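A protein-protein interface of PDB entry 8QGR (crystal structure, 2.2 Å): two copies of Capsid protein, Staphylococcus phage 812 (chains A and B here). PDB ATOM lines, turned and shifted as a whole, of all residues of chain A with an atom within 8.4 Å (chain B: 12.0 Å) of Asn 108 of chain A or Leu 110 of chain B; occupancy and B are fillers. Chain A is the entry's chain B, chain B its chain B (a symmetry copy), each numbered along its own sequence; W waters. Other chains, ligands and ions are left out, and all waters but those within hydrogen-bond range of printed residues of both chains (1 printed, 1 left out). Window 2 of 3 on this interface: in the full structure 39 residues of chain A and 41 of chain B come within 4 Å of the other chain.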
ATOM      1  N   SER A 102       1.459  19.496 -13.979  1.00  0.00           N
ATOM      2  CA  SER A 102       2.815  19.812 -14.396  1.00  0.00           C
ATOM      3  C   SER A 102       2.998  21.327 -14.503  1.00  0.00           C
ATOM      4  O   SER A 102       4.098  21.792 -14.790  1.00  0.00           O
ATOM      5  CB  SER A 102       3.168  19.096 -15.677  1.00  0.00           C
ATOM      6  OG  SER A 102       2.179  19.326 -16.667  1.00  0.00           O
ATOM      7  N   GLN A 103       1.927  22.088 -14.241  1.00  0.00           N
ATOM      8  CA  GLN A 103       1.966  23.541 -14.311  1.00  0.00           C
ATOM      9  C   GLN A 103       1.146  24.123 -13.165  1.00  0.00           C
ATOM     10  O   GLN A 103       0.067  23.623 -12.871  1.00  0.00           O
ATOM     11  CB  GLN A 103       1.340  24.084 -15.599  1.00  0.00           C
ATOM     12  CG  GLN A 103       2.026  23.654 -16.885  1.00  0.00           C
ATOM     13  CD  GLN A 103       1.291  24.125 -18.117  1.00  0.00           C
ATOM     14  OE1 GLN A 103       0.695  23.331 -18.838  1.00  0.00           O
ATOM     15  NE2 GLN A 103       1.316  25.424 -18.372  1.00  0.00           N
ATOM     16  N   GLU A 104       1.656  25.190 -12.545  1.00  0.00           N
ATOM     17  CA  GLU A 104       0.918  25.915 -11.523  1.00  0.00           C
ATOM     18  C   GLU A 104       1.559  27.282 -11.311  1.00  0.00           C
ATOM     19  O   GLU A 104       2.661  27.527 -11.789  1.00  0.00           O
ATOM     20  CB  GLU A 104       0.896  25.155 -10.199  1.00  0.00           C
ATOM     21  CG  GLU A 104       2.271  24.933  -9.612  1.00  0.00           C
ATOM     22  CD  GLU A 104       2.268  24.661  -8.117  1.00  0.00           C
ATOM     23  OE1 GLU A 104       1.540  23.749  -7.684  1.00  0.00           O
ATOM     24  OE2 GLU A 104       3.001  25.366  -7.390  1.00  0.00           O
ATOM     25  N   LYS A 105       0.877  28.162 -10.572  1.00  0.00           N
ATOM     26  CA  LYS A 105       1.400  29.502 -10.351  1.00  0.00           C
ATOM     27  C   LYS A 105       2.806  29.402  -9.767  1.00  0.00           C
ATOM     28  O   LYS A 105       3.691  30.201 -10.088  1.00  0.00           O
ATOM     29  CB  LYS A 105       0.478  30.307  -9.430  1.00  0.00           C
ATOM     30  CG  LYS A 105       0.876  31.770  -9.254  1.00  0.00           C
ATOM     31  CD  LYS A 105      -0.097  32.545  -8.395  1.00  0.00           C
ATOM     32  CE  LYS A 105       0.325  33.978  -8.155  1.00  0.00           C
ATOM     33  NZ  LYS A 105      -0.612  34.664  -7.232  1.00  0.00           N
ATOM     34  N   GLY A 106       2.999  28.375  -8.932  1.00  0.00           N
ATOM     35  CA  GLY A 106       4.273  28.134  -8.277  1.00  0.00           C
ATOM     36  C   GLY A 106       5.404  27.829  -9.253  1.00  0.00           C
ATOM     37  O   GLY A 106       6.554  27.824  -8.848  1.00  0.00           O
ATOM     38  N   THR A 107       5.079  27.559 -10.527  1.00  0.00           N
ATOM     39  CA  THR A 107       6.096  27.304 -11.538  1.00  0.00           C
ATOM     40  C   THR A 107       5.998  28.365 -12.630  1.00  0.00           C
ATOM     41  O   THR A 107       6.623  28.226 -13.676  1.00  0.00           O
ATOM     42  CB  THR A 107       5.954  25.907 -12.166  1.00  0.00           C
ATOM     43  OG1 THR A 107       4.788  25.883 -12.991  1.00  0.00           O
ATOM     44  CG2 THR A 107       5.847  24.803 -11.138  1.00  0.00           C
ATOM     45  N   ASN A 108       5.187  29.404 -12.393  1.00  0.00           N
ATOM     46  CA  ASN A 108       5.025  30.487 -13.354  1.00  0.00           C
ATOM     47  C   ASN A 108       4.227  29.933 -14.537  1.00  0.00           C
ATOM     48  O   ASN A 108       4.306  30.434 -15.655  1.00  0.00           O
ATOM     49  CB  ASN A 108       6.399  31.093 -13.679  1.00  0.00           C
ATOM     50  CG  ASN A 108       6.362  32.368 -14.498  1.00  0.00           C
ATOM     51  OD1 ASN A 108       5.563  33.262 -14.232  1.00  0.00           O
ATOM     52  ND2 ASN A 108       7.228  32.467 -15.496  1.00  0.00           N
ATOM     53  N   GLN A 109       3.443  28.884 -14.261  1.00  0.00           N
ATOM     54  CA  GLN A 109       2.665  28.170 -15.265  1.00  0.00           C
ATOM     55  C   GLN A 109       3.575  27.510 -16.301  1.00  0.00           C
ATOM     56  O   GLN A 109       3.092  27.067 -17.338  1.00  0.00           O
ATOM     57  CB  GLN A 109       1.633  29.090 -15.926  1.00  0.00           C
ATOM     58  CG  GLN A 109       0.480  29.467 -15.003  1.00  0.00           C
ATOM     59  CD  GLN A 109      -0.335  28.275 -14.563  1.00  0.00           C
ATOM     60  OE1 GLN A 109      -0.217  27.172 -15.092  1.00  0.00           O
ATOM     61  NE2 GLN A 109      -1.191  28.488 -13.582  1.00  0.00           N
ATOM     62  N   LEU A 110       4.880  27.440 -16.014  1.00  0.00           N
ATOM     63  CA  LEU A 110       5.801  26.653 -16.824  1.00  0.00           C
ATOM     64  C   LEU A 110       5.573  25.176 -16.532  1.00  0.00           C
ATOM     65  O   LEU A 110       5.197  24.809 -15.413  1.00  0.00           O
ATOM     66  CB  LEU A 110       7.249  27.030 -16.498  1.00  0.00           C
ATOM     67  CG  LEU A 110       7.684  28.410 -16.982  1.00  0.00           C
ATOM     68  CD1 LEU A 110       9.084  28.743 -16.496  1.00  0.00           C
ATOM     69  CD2 LEU A 110       7.624  28.479 -18.497  1.00  0.00           C
ATOM     70  N   ASP A 111       5.829  24.351 -17.557  1.00  0.00           N
ATOM     71  CA  ASP A 111       5.657  22.913 -17.473  1.00  0.00           C
ATOM     72  C   ASP A 111       6.916  22.308 -16.863  1.00  0.00           C
ATOM     73  O   ASP A 111       7.930  22.124 -17.533  1.00  0.00           O
ATOM     74  CB  ASP A 111       5.341  22.295 -18.840  1.00  0.00           C
ATOM     75  CG  ASP A 111       4.865  20.852 -18.747  1.00  0.00           C
ATOM     76  OD1 ASP A 111       5.591  20.029 -18.148  1.00  0.00           O
ATOM     77  OD2 ASP A 111       3.765  20.560 -19.268  1.00  0.00           O
ATOM     78  N   ILE A 112       6.820  21.939 -15.586  1.00  0.00           N
ATOM     79  CA  ILE A 112       7.961  21.397 -14.865  1.00  0.00           C
ATOM     80  C   ILE A 112       8.426  20.078 -15.499  1.00  0.00           C
ATOM     81  O   ILE A 112       9.594  19.708 -15.378  1.00  0.00           O
ATOM     82  CB  ILE A 112       7.612  21.270 -13.370  1.00  0.00           C
ATOM     83  CG1 ILE A 112       8.854  21.042 -12.508  1.00  0.00           C
ATOM     84  CG2 ILE A 112       6.550  20.201 -13.145  1.00  0.00           C
ATOM     85  CD1 ILE A 112       8.573  21.129 -11.022  1.00  0.00           C
ATOM     86  N   LEU A 115      10.789  21.250 -18.079  1.00  0.00           N
ATOM     87  CA  LEU A 115      11.973  21.734 -17.390  1.00  0.00           C
ATOM     88  C   LEU A 115      12.790  20.548 -16.887  1.00  0.00           C
ATOM     89  O   LEU A 115      14.011  20.561 -16.971  1.00  0.00           O
ATOM     90  CB  LEU A 115      11.563  22.629 -16.216  1.00  0.00           C
ATOM     91  CG  LEU A 115      10.737  23.866 -16.570  1.00  0.00           C
ATOM     92  CD1 LEU A 115      10.496  24.729 -15.341  1.00  0.00           C
ATOM     93  CD2 LEU A 115      11.409  24.687 -17.653  1.00  0.00           C
ATOM     94  N   LYS A 219       5.079  22.923   0.723  1.00  0.00           N
ATOM     95  CA  LYS A 219       4.150  23.632   1.596  1.00  0.00           C
ATOM     96  C   LYS A 219       3.965  22.897   2.919  1.00  0.00           C
ATOM     97  O   LYS A 219       2.841  22.783   3.388  1.00  0.00           O
ATOM     98  CB  LYS A 219       2.743  23.705   0.996  1.00  0.00           C
ATOM     99  CG  LYS A 219       2.643  24.231  -0.425  1.00  0.00           C
ATOM    100  CD  LYS A 219       3.024  25.667  -0.570  1.00  0.00           C
ATOM    101  CE  LYS A 219       2.772  26.154  -1.979  1.00  0.00           C
ATOM    102  NZ  LYS A 219       3.302  27.519  -2.186  1.00  0.00           N
ATOM    103  N   ILE B 100       4.966  31.425   7.589  1.00  0.00           N
ATOM    104  CA  ILE B 100       5.884  30.688   6.738  1.00  0.00           C
ATOM    105  C   ILE B 100       5.309  30.641   5.322  1.00  0.00           C
ATOM    106  O   ILE B 100       4.160  30.248   5.147  1.00  0.00           O
ATOM    107  CB  ILE B 100       6.129  29.280   7.309  1.00  0.00           C
ATOM    108  CG1 ILE B 100       6.760  29.351   8.702  1.00  0.00           C
ATOM    109  CG2 ILE B 100       6.965  28.442   6.352  1.00  0.00           C
ATOM    110  CD1 ILE B 100       6.923  28.014   9.372  1.00  0.00           C
ATOM    111  N   GLN B 101       6.114  31.035   4.324  1.00  0.00           N
ATOM    112  CA  GLN B 101       5.674  31.034   2.939  1.00  0.00           C
ATOM    113  C   GLN B 101       6.744  30.432   2.035  1.00  0.00           C
ATOM    114  O   GLN B 101       7.932  30.485   2.338  1.00  0.00           O
ATOM    115  CB  GLN B 101       5.455  32.453   2.416  1.00  0.00           C
ATOM    116  CG  GLN B 101       4.801  33.394   3.407  1.00  0.00           C
ATOM    117  CD  GLN B 101       4.895  34.806   2.883  1.00  0.00           C
ATOM    118  OE1 GLN B 101       5.734  35.603   3.311  1.00  0.00           O
ATOM    119  NE2 GLN B 101       4.081  35.094   1.882  1.00  0.00           N
ATOM    120  N   SER B 102       6.313  29.922   0.882  1.00  0.00           N
ATOM    121  CA  SER B 102       7.248  29.437  -0.118  1.00  0.00           C
ATOM    122  C   SER B 102       7.125  30.258  -1.403  1.00  0.00           C
ATOM    123  O   SER B 102       7.876  30.033  -2.348  1.00  0.00           O
ATOM    124  CB  SER B 102       7.067  27.958  -0.359  1.00  0.00           C
ATOM    125  OG  SER B 102       5.707  27.660  -0.631  1.00  0.00           O
ATOM    126  N   GLN B 103       6.199  31.226  -1.418  1.00  0.00           N
ATOM    127  CA  GLN B 103       5.975  32.075  -2.579  1.00  0.00           C
ATOM    128  C   GLN B 103       5.709  33.503  -2.115  1.00  0.00           C
ATOM    129  O   GLN B 103       4.985  33.705  -1.148  1.00  0.00           O
ATOM    130  CB  GLN B 103       4.744  31.655  -3.387  1.00  0.00           C
ATOM    131  CG  GLN B 103       4.806  30.258  -3.983  1.00  0.00           C
ATOM    132  CD  GLN B 103       3.516  29.863  -4.664  1.00  0.00           C
ATOM    133  OE1 GLN B 103       2.783  29.009  -4.178  1.00  0.00           O
ATOM    134  NE2 GLN B 103       3.219  30.486  -5.794  1.00  0.00           N
ATOM    135  N   GLU B 104       6.278  34.479  -2.824  1.00  0.00           N
ATOM    136  CA  GLU B 104       6.003  35.884  -2.565  1.00  0.00           C
ATOM    137  C   GLU B 104       6.450  36.716  -3.762  1.00  0.00           C
ATOM    138  O   GLU B 104       7.147  36.213  -4.636  1.00  0.00           O
ATOM    139  CB  GLU B 104       6.721  36.375  -1.310  1.00  0.00           C
ATOM    140  CG  GLU B 104       8.226  36.277  -1.403  1.00  0.00           C
ATOM    141  CD  GLU B 104       8.965  37.195  -0.443  1.00  0.00           C
ATOM    142  OE1 GLU B 104       8.674  37.141   0.766  1.00  0.00           O
ATOM    143  OE2 GLU B 104       9.834  37.960  -0.913  1.00  0.00           O
ATOM    144  N   LYS B 105       6.067  37.996  -3.786  1.00  0.00           N
ATOM    145  CA  LYS B 105       6.419  38.851  -4.911  1.00  0.00           C
ATOM    146  C   LYS B 105       7.931  38.819  -5.110  1.00  0.00           C
ATOM    147  O   LYS B 105       8.428  38.839  -6.240  1.00  0.00           O
ATOM    148  CB  LYS B 105       5.923  40.283  -4.689  1.00  0.00           C
ATOM    149  CG  LYS B 105       6.128  41.217  -5.878  1.00  0.00           C
ATOM    150  CD  LYS B 105       5.563  42.600  -5.644  1.00  0.00           C
ATOM    151  CE  LYS B 105       5.822  43.554  -6.788  1.00  0.00           C
ATOM    152  NZ  LYS B 105       5.333  44.918  -6.469  1.00  0.00           N
ATOM    153  N   GLY B 106       8.648  38.727  -3.985  1.00  0.00           N
ATOM    154  CA  GLY B 106      10.100  38.695  -3.987  1.00  0.00           C
ATOM    155  C   GLY B 106      10.674  37.478  -4.705  1.00  0.00           C
ATOM    156  O   GLY B 106      11.866  37.448  -4.963  1.00  0.00           O
ATOM    157  N   THR B 107       9.837  36.474  -5.007  1.00  0.00           N
ATOM    158  CA  THR B 107      10.288  35.294  -5.732  1.00  0.00           C
ATOM    159  C   THR B 107       9.528  35.193  -7.052  1.00  0.00           C
ATOM    160  O   THR B 107       9.604  34.171  -7.725  1.00  0.00           O
ATOM    161  CB  THR B 107      10.086  34.002  -4.924  1.00  0.00           C
ATOM    162  OG1 THR B 107       8.688  33.713  -4.848  1.00  0.00           O
ATOM    163  CG2 THR B 107      10.643  34.087  -3.521  1.00  0.00           C
ATOM    164  N   ASN B 108       8.773  36.244  -7.397  1.00  0.00           N
ATOM    165  CA  ASN B 108       8.016  36.271  -8.641  1.00  0.00           C
ATOM    166  C   ASN B 108       6.853  35.287  -8.489  1.00  0.00           C
ATOM    167  O   ASN B 108       6.322  34.766  -9.466  1.00  0.00           O
ATOM    168  CB  ASN B 108       8.966  36.030  -9.825  1.00  0.00           C
ATOM    169  CG  ASN B 108       8.355  36.245 -11.196  1.00  0.00           C
ATOM    170  OD1 ASN B 108       7.646  37.222 -11.420  1.00  0.00           O
ATOM    171  ND2 ASN B 108       8.626  35.339 -12.124  1.00  0.00           N
ATOM    172  N   GLN B 109       6.462  35.049  -7.232  1.00  0.00           N
ATOM    173  CA  GLN B 109       5.424  34.089  -6.876  1.00  0.00           C
ATOM    174  C   GLN B 109       5.834  32.668  -7.262  1.00  0.00           C
ATOM    175  O   GLN B 109       4.996  31.770  -7.249  1.00  0.00           O
ATOM    176  CB  GLN B 109       4.075  34.474  -7.492  1.00  0.00           C
ATOM    177  CG  GLN B 109       3.447  35.705  -6.849  1.00  0.00           C
ATOM    178  CD  GLN B 109       3.127  35.505  -5.387  1.00  0.00           C
ATOM    179  OE1 GLN B 109       3.151  34.396  -4.858  1.00  0.00           O
ATOM    180  NE2 GLN B 109       2.808  36.591  -4.711  1.00  0.00           N
ATOM    181  N   LEU B 110       7.114  32.466  -7.593  1.00  0.00           N
ATOM    182  CA  LEU B 110       7.657  31.127  -7.772  1.00  0.00           C
ATOM    183  C   LEU B 110       7.823  30.476  -6.406  1.00  0.00           C
ATOM    184  O   LEU B 110       8.076  31.165  -5.410  1.00  0.00           O
ATOM    185  CB  LEU B 110       9.012  31.194  -8.484  1.00  0.00           C
ATOM    186  CG  LEU B 110       8.952  31.586  -9.958  1.00  0.00           C
ATOM    187  CD1 LEU B 110      10.346  31.757 -10.534  1.00  0.00           C
ATOM    188  CD2 LEU B 110       8.180  30.545 -10.747  1.00  0.00           C
ATOM    189  N   ASP B 111       7.694  29.142  -6.395  1.00  0.00           N
ATOM    190  CA  ASP B 111       7.804  28.349  -5.185  1.00  0.00           C
ATOM    191  C   ASP B 111       9.279  28.061  -4.927  1.00  0.00           C
ATOM    192  O   ASP B 111       9.876  27.175  -5.535  1.00  0.00           O
ATOM    193  CB  ASP B 111       6.984  27.057  -5.273  1.00  0.00           C
ATOM    194  CG  ASP B 111       6.836  26.353  -3.931  1.00  0.00           C
ATOM    195  OD1 ASP B 111       7.875  26.068  -3.296  1.00  0.00           O
ATOM    196  OD2 ASP B 111       5.680  26.099  -3.523  1.00  0.00           O
ATOM    197  N   ILE B 112       9.849  28.785  -3.965  1.00  0.00           N
ATOM    198  CA  ILE B 112      11.263  28.649  -3.651  1.00  0.00           C
ATOM    199  C   ILE B 112      11.575  27.231  -3.151  1.00  0.00           C
ATOM    200  O   ILE B 112      12.704  26.761  -3.281  1.00  0.00           O
ATOM    201  CB  ILE B 112      11.679  29.754  -2.661  1.00  0.00           C
ATOM    202  CG1 ILE B 112      13.198  29.890  -2.557  1.00  0.00           C
ATOM    203  CG2 ILE B 112      11.024  29.544  -1.301  1.00  0.00           C
ATOM    204  CD1 ILE B 112      13.635  31.103  -1.763  1.00  0.00           C
ATOM    205  N   GLY B 113      10.567  26.539  -2.603  1.00  0.00           N
ATOM    206  CA  GLY B 113      10.721  25.160  -2.153  1.00  0.00           C
ATOM    207  C   GLY B 113      10.894  24.174  -3.312  1.00  0.00           C
ATOM    208  O   GLY B 113      11.458  23.099  -3.133  1.00  0.00           O
ATOM    209  N   ILE B 114      10.380  24.540  -4.498  1.00  0.00           N
ATOM    210  CA  ILE B 114      10.582  23.749  -5.703  1.00  0.00           C
ATOM    211  C   ILE B 114      11.934  24.129  -6.297  1.00  0.00           C
ATOM    212  O   ILE B 114      12.675  23.271  -6.754  1.00  0.00           O
ATOM    213  CB  ILE B 114       9.434  23.954  -6.717  1.00  0.00           C
ATOM    214  CG1 ILE B 114       8.081  23.530  -6.142  1.00  0.00           C
ATOM    215  CG2 ILE B 114       9.726  23.228  -8.020  1.00  0.00           C
ATOM    216  CD1 ILE B 114       6.905  23.815  -7.052  1.00  0.00           C
ATOM    217  N   LEU B 115      12.243  25.429  -6.300  1.00  0.00           N
ATOM    218  CA  LEU B 115      13.520  25.902  -6.804  1.00  0.00           C
ATOM    219  C   LEU B 115      14.650  25.295  -5.977  1.00  0.00           C
ATOM    220  O   LEU B 115      15.671  24.901  -6.524  1.00  0.00           O
ATOM    221  CB  LEU B 115      13.575  27.432  -6.731  1.00  0.00           C
ATOM    222  CG  LEU B 115      12.500  28.181  -7.519  1.00  0.00           C
ATOM    223  CD1 LEU B 115      12.733  29.683  -7.461  1.00  0.00           C
ATOM    224  CD2 LEU B 115      12.453  27.721  -8.962  1.00  0.00           C
ATOM    225  N   ASP B 116      14.467  25.208  -4.657  1.00  0.00           N
ATOM    226  CA  ASP B 116      15.552  24.743  -3.804  1.00  0.00           C
ATOM    227  C   ASP B 116      14.986  23.952  -2.624  1.00  0.00           C
ATOM    228  O   ASP B 116      14.414  24.525  -1.703  1.00  0.00           O
ATOM    229  CB  ASP B 116      16.390  25.943  -3.372  1.00  0.00           C
ATOM    230  CG  ASP B 116      17.712  25.573  -2.730  1.00  0.00           C
ATOM    231  OD1 ASP B 116      18.062  24.370  -2.738  1.00  0.00           O
ATOM    232  OD2 ASP B 116      18.373  26.493  -2.214  1.00  0.00           O
ATOM    233  N   THR B 117      15.177  22.628  -2.643  1.00  0.00           N
ATOM    234  CA  THR B 117      14.525  21.756  -1.683  1.00  0.00           C
ATOM    235  C   THR B 117      14.733  22.254  -0.250  1.00  0.00           C
ATOM    236  O   THR B 117      15.848  22.509   0.203  1.00  0.00           O
ATOM    237  CB  THR B 117      14.946  20.286  -1.852  1.00  0.00           C
ATOM    238  OG1 THR B 117      14.216  19.516  -0.896  1.00  0.00           O
ATOM    239  CG2 THR B 117      16.424  20.040  -1.655  1.00  0.00           C
ATOM    240  N   GLY B 118      13.619  22.372   0.463  1.00  0.00           N
ATOM    241  CA  GLY B 118      13.654  22.651   1.890  1.00  0.00           C
ATOM    242  C   GLY B 118      13.822  24.135   2.212  1.00  0.00           C
ATOM    243  O   GLY B 118      14.151  24.478   3.341  1.00  0.00           O
ATOM    244  N   THR B 119      13.563  25.013   1.236  1.00  0.00           N
ATOM    245  CA  THR B 119      13.709  26.441   1.457  1.00  0.00           C
ATOM    246  C   THR B 119      12.333  27.052   1.667  1.00  0.00           C
ATOM    247  O   THR B 119      11.362  26.705   0.994  1.00  0.00           O
ATOM    248  CB  THR B 119      14.454  27.135   0.309  1.00  0.00           C
ATOM    249  OG1 THR B 119      15.657  26.427   0.004  1.00  0.00           O
ATOM    250  CG2 THR B 119      14.797  28.572   0.631  1.00  0.00           C
ATOM    251  N   ALA B 120      12.260  27.952   2.643  1.00  0.00           N
ATOM    252  CA  ALA B 120      11.052  28.712   2.907  1.00  0.00           C
ATOM    253  C   ALA B 120      11.452  30.078   3.454  1.00  0.00           C
ATOM    254  O   ALA B 120      12.601  30.298   3.819  1.00  0.00           O
ATOM    255  CB  ALA B 120      10.176  27.965   3.882  1.00  0.00           C
ATOM    256  N   ILE B 121      10.470  30.972   3.524  1.00  0.00           N
ATOM    257  CA  ILE B 121      10.652  32.310   4.040  1.00  0.00           C
ATOM    258  C   ILE B 121       9.787  32.450   5.291  1.00  0.00           C
ATOM    259  O   ILE B 121       8.593  32.142   5.269  1.00  0.00           O
ATOM    260  CB  ILE B 121      10.281  33.320   2.934  1.00  0.00           C
ATOM    261  CG1 ILE B 121      11.155  33.101   1.698  1.00  0.00           C
ATOM    262  CG2 ILE B 121      10.356  34.750   3.435  1.00  0.00           C
ATOM    263  CD1 ILE B 121      10.612  33.740   0.442  1.00  0.00           C
ATOM    264  N   LEU B 218      16.768  38.635   5.800  1.00  0.00           N
ATOM    265  CA  LEU B 218      16.334  39.405   4.638  1.00  0.00           C
ATOM    266  C   LEU B 218      15.767  40.752   5.086  1.00  0.00           C
ATOM    267  O   LEU B 218      15.288  40.884   6.213  1.00  0.00           O
ATOM    268  CB  LEU B 218      15.262  38.601   3.893  1.00  0.00           C
ATOM    269  CG  LEU B 218      15.665  37.187   3.472  1.00  0.00           C
ATOM    270  CD1 LEU B 218      14.474  36.419   2.916  1.00  0.00           C
ATOM    271  CD2 LEU B 218      16.784  37.240   2.450  1.00  0.00           C
ATOM    272  N   LYS B 241      12.529  39.034   9.013  1.00  0.00           N
ATOM    273  CA  LYS B 241      12.264  38.181   7.872  1.00  0.00           C
ATOM    274  C   LYS B 241      13.494  37.320   7.613  1.00  0.00           C
ATOM    275  O   LYS B 241      14.612  37.834   7.562  1.00  0.00           O
ATOM    276  CB  LYS B 241      11.838  39.051   6.690  1.00  0.00           C
ATOM    277  CG  LYS B 241      11.489  38.290   5.427  1.00  0.00           C
ATOM    278  CD  LYS B 241      10.818  39.179   4.432  1.00  0.00           C
ATOM    279  CE  LYS B 241      10.403  38.470   3.166  1.00  0.00           C
ATOM    280  NZ  LYS B 241       9.687  39.414   2.274  1.00  0.00           N
ATOM    281  N   LEU B 243      15.331  33.669   5.728  1.00  0.00           N
ATOM    282  CA  LEU B 243      15.381  32.551   4.809  1.00  0.00           C
ATOM    283  C   LEU B 243      15.606  31.290   5.645  1.00  0.00           C
ATOM    284  O   LEU B 243      16.517  31.233   6.467  1.00  0.00           O
ATOM    285  CB  LEU B 243      16.500  32.779   3.793  1.00  0.00           C
ATOM    286  CG  LEU B 243      16.462  31.883   2.558  1.00  0.00           C
ATOM    287  CD1 LEU B 243      15.205  32.136   1.736  1.00  0.00           C
ATOM    288  CD2 LEU B 243      17.701  32.097   1.692  1.00  0.00           C
HETATM  289  O   HOH W   1       7.036  24.448  -0.900  1.00  0.00           O
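The backbone NH (N) of Asp 111 of chain B is in hydrogen-bond range of the backbone carbonyl oxygen (O) of Gly 106 of chain A.
OG of Ser 102 of chain B sits at hydrogen-bond distance from NZ of Lys 219 of chain A.
NZ of Lys 219 of chain A sits at hydrogen-bond distance from OE1 of Gln 103 of chain B, at 2.5 Å.
OD2 of Asp 111 of chain B is in salt-bridge range of NZ of Lys 219 of chain A, 3.1 Å away.
The backbone carbonyl oxygen (O) of Gln 109 of chain B sits close to the backbone carbonyl oxygen (O) of Lys 105 of chain A, 3.5 Å away.
OE2 of Glu 104 of chain A lies close to N of Gly 106 of chain A (3.4 Å).
The backbone carbonyl oxygen (O) of Glu 104 of chain A sits at hydrogen-bond distance from the side-chain hydroxyl (OG1) of Thr 107 of chain A, 2.9 Å away.
The side-chain hydroxyl of Thr 107 of chain A lies within hydrogen-bond range of the backbone carbonyl oxygen of Leu 110 of chain A.
The side-chain amide nitrogen (NE2) of Gln 101 of chain B lies within hydrogen-bond range of the backbone carbonyl oxygen (O) of Gln 103 of chain B, 3.5 Å away.
The backbone carbonyl oxygen (O) of Ser 102 of chain B is in hydrogen-bond range of the backbone NH (N) of Ile 112 of chain B.
N of Gln 109 of chain B lies within hydrogen-bond range of O of Glu 104 of chain B, 2.9 Å away.
Among the printed residues, pairs that only touch across the chains: Asn 108 of chain A with Leu 110 of chain B (3.5 Å), Gly 106 of chain A with Gln 103 of chain B (3.6 Å), Thr 107 of chain A with Leu 110 of chain B (3.6 Å), Gly 106 of chain A with Leu 110 of chain B (3.6 Å), Ile 112 of chain A with Ile 114 of chain B (3.8 Å) and Gly 106 of chain A with Gln 109 of chain B (3.8 Å).
Of the printed residues of chain B, Lys 105 of chain A touches Gln 109.
Gly 106 of chain A touches four residues of chain B.
Thr 107 of chain A touches one residue of chain B.
Asn 108 of chain A touches one residue of chain B.
No residue of chain B comes within 4 Å of Gln 109 of chain A.
No residue of chain B comes within 4 Å of Leu 110 of chain A.
Of the printed residues of chain B, Ile 112 of chain A touches Ile 114 (3.8 Å).
Of the printed residues of chain A, Ser 102 of chain B touches Lys 219.
Glu 104 of chain B touches none of the printed residues of chain A.
Of the printed residues of chain A, Gln 109 of chain B touches Lys 105 (3.5 Å) and Gly 106 (3.8 Å).
Printed residues of chain A within 4 Å of Leu 110 of chain B: Gly 106, Thr 107 and Asn 108.
Printed residues of chain A within 4 Å of Asp 111 of chain B: Gly 106 (3.0 Å) and Lys 219 (3.1 Å).
Asp 116 of chain B touches none of the printed residues of chain A.
The nearest residue of chain B that does not touch Asn 108 of chain A is Asn 108 of chain B (4.3 Å).
Of the 13 printed residues of chain A, 6 touch a printed residue of chain B.
Printed residues of chain A that touch a printed residue of chain B: Lys 105, Gly 106, Thr 107, Asn 108, Ile 112 and Lys 219.
Of the 25 printed residues of chain B, 6 touch a printed residue of chain A.
Gly 106 of chain A touches Gln 103 of chain B, but with the chains exchanged Gln 103 of chain A does not touch Gly 106 of chain B (18.5 Å).
Gly 106 of chain A touches Asp 111 of chain B, but with the chains exchanged Asp 111 of chain A does not touch Gly 106 of chain B (19.0 Å).
Thr 107 of chain A touches Leu 110 of chain B, but with the chains exchanged Leu 110 of chain A does not touch Thr 107 of chain B (10.3 Å).
Asn 108 of chain A touches Leu 110 of chain B, but with the chains exchanged Leu 110 of chain A does not touch Asn 108 of chain B (7.9 Å).
12 positions are printed for both chains.
Water W1 lies within hydrogen-bond range of the backbone NH of Lys 219 of chain A (3.0 Å), the side-chain carboxylate of Asp 111 of chain B (3.0 Å) and the side-chain hydroxyl of Ser 102 of chain B (3.5 Å).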
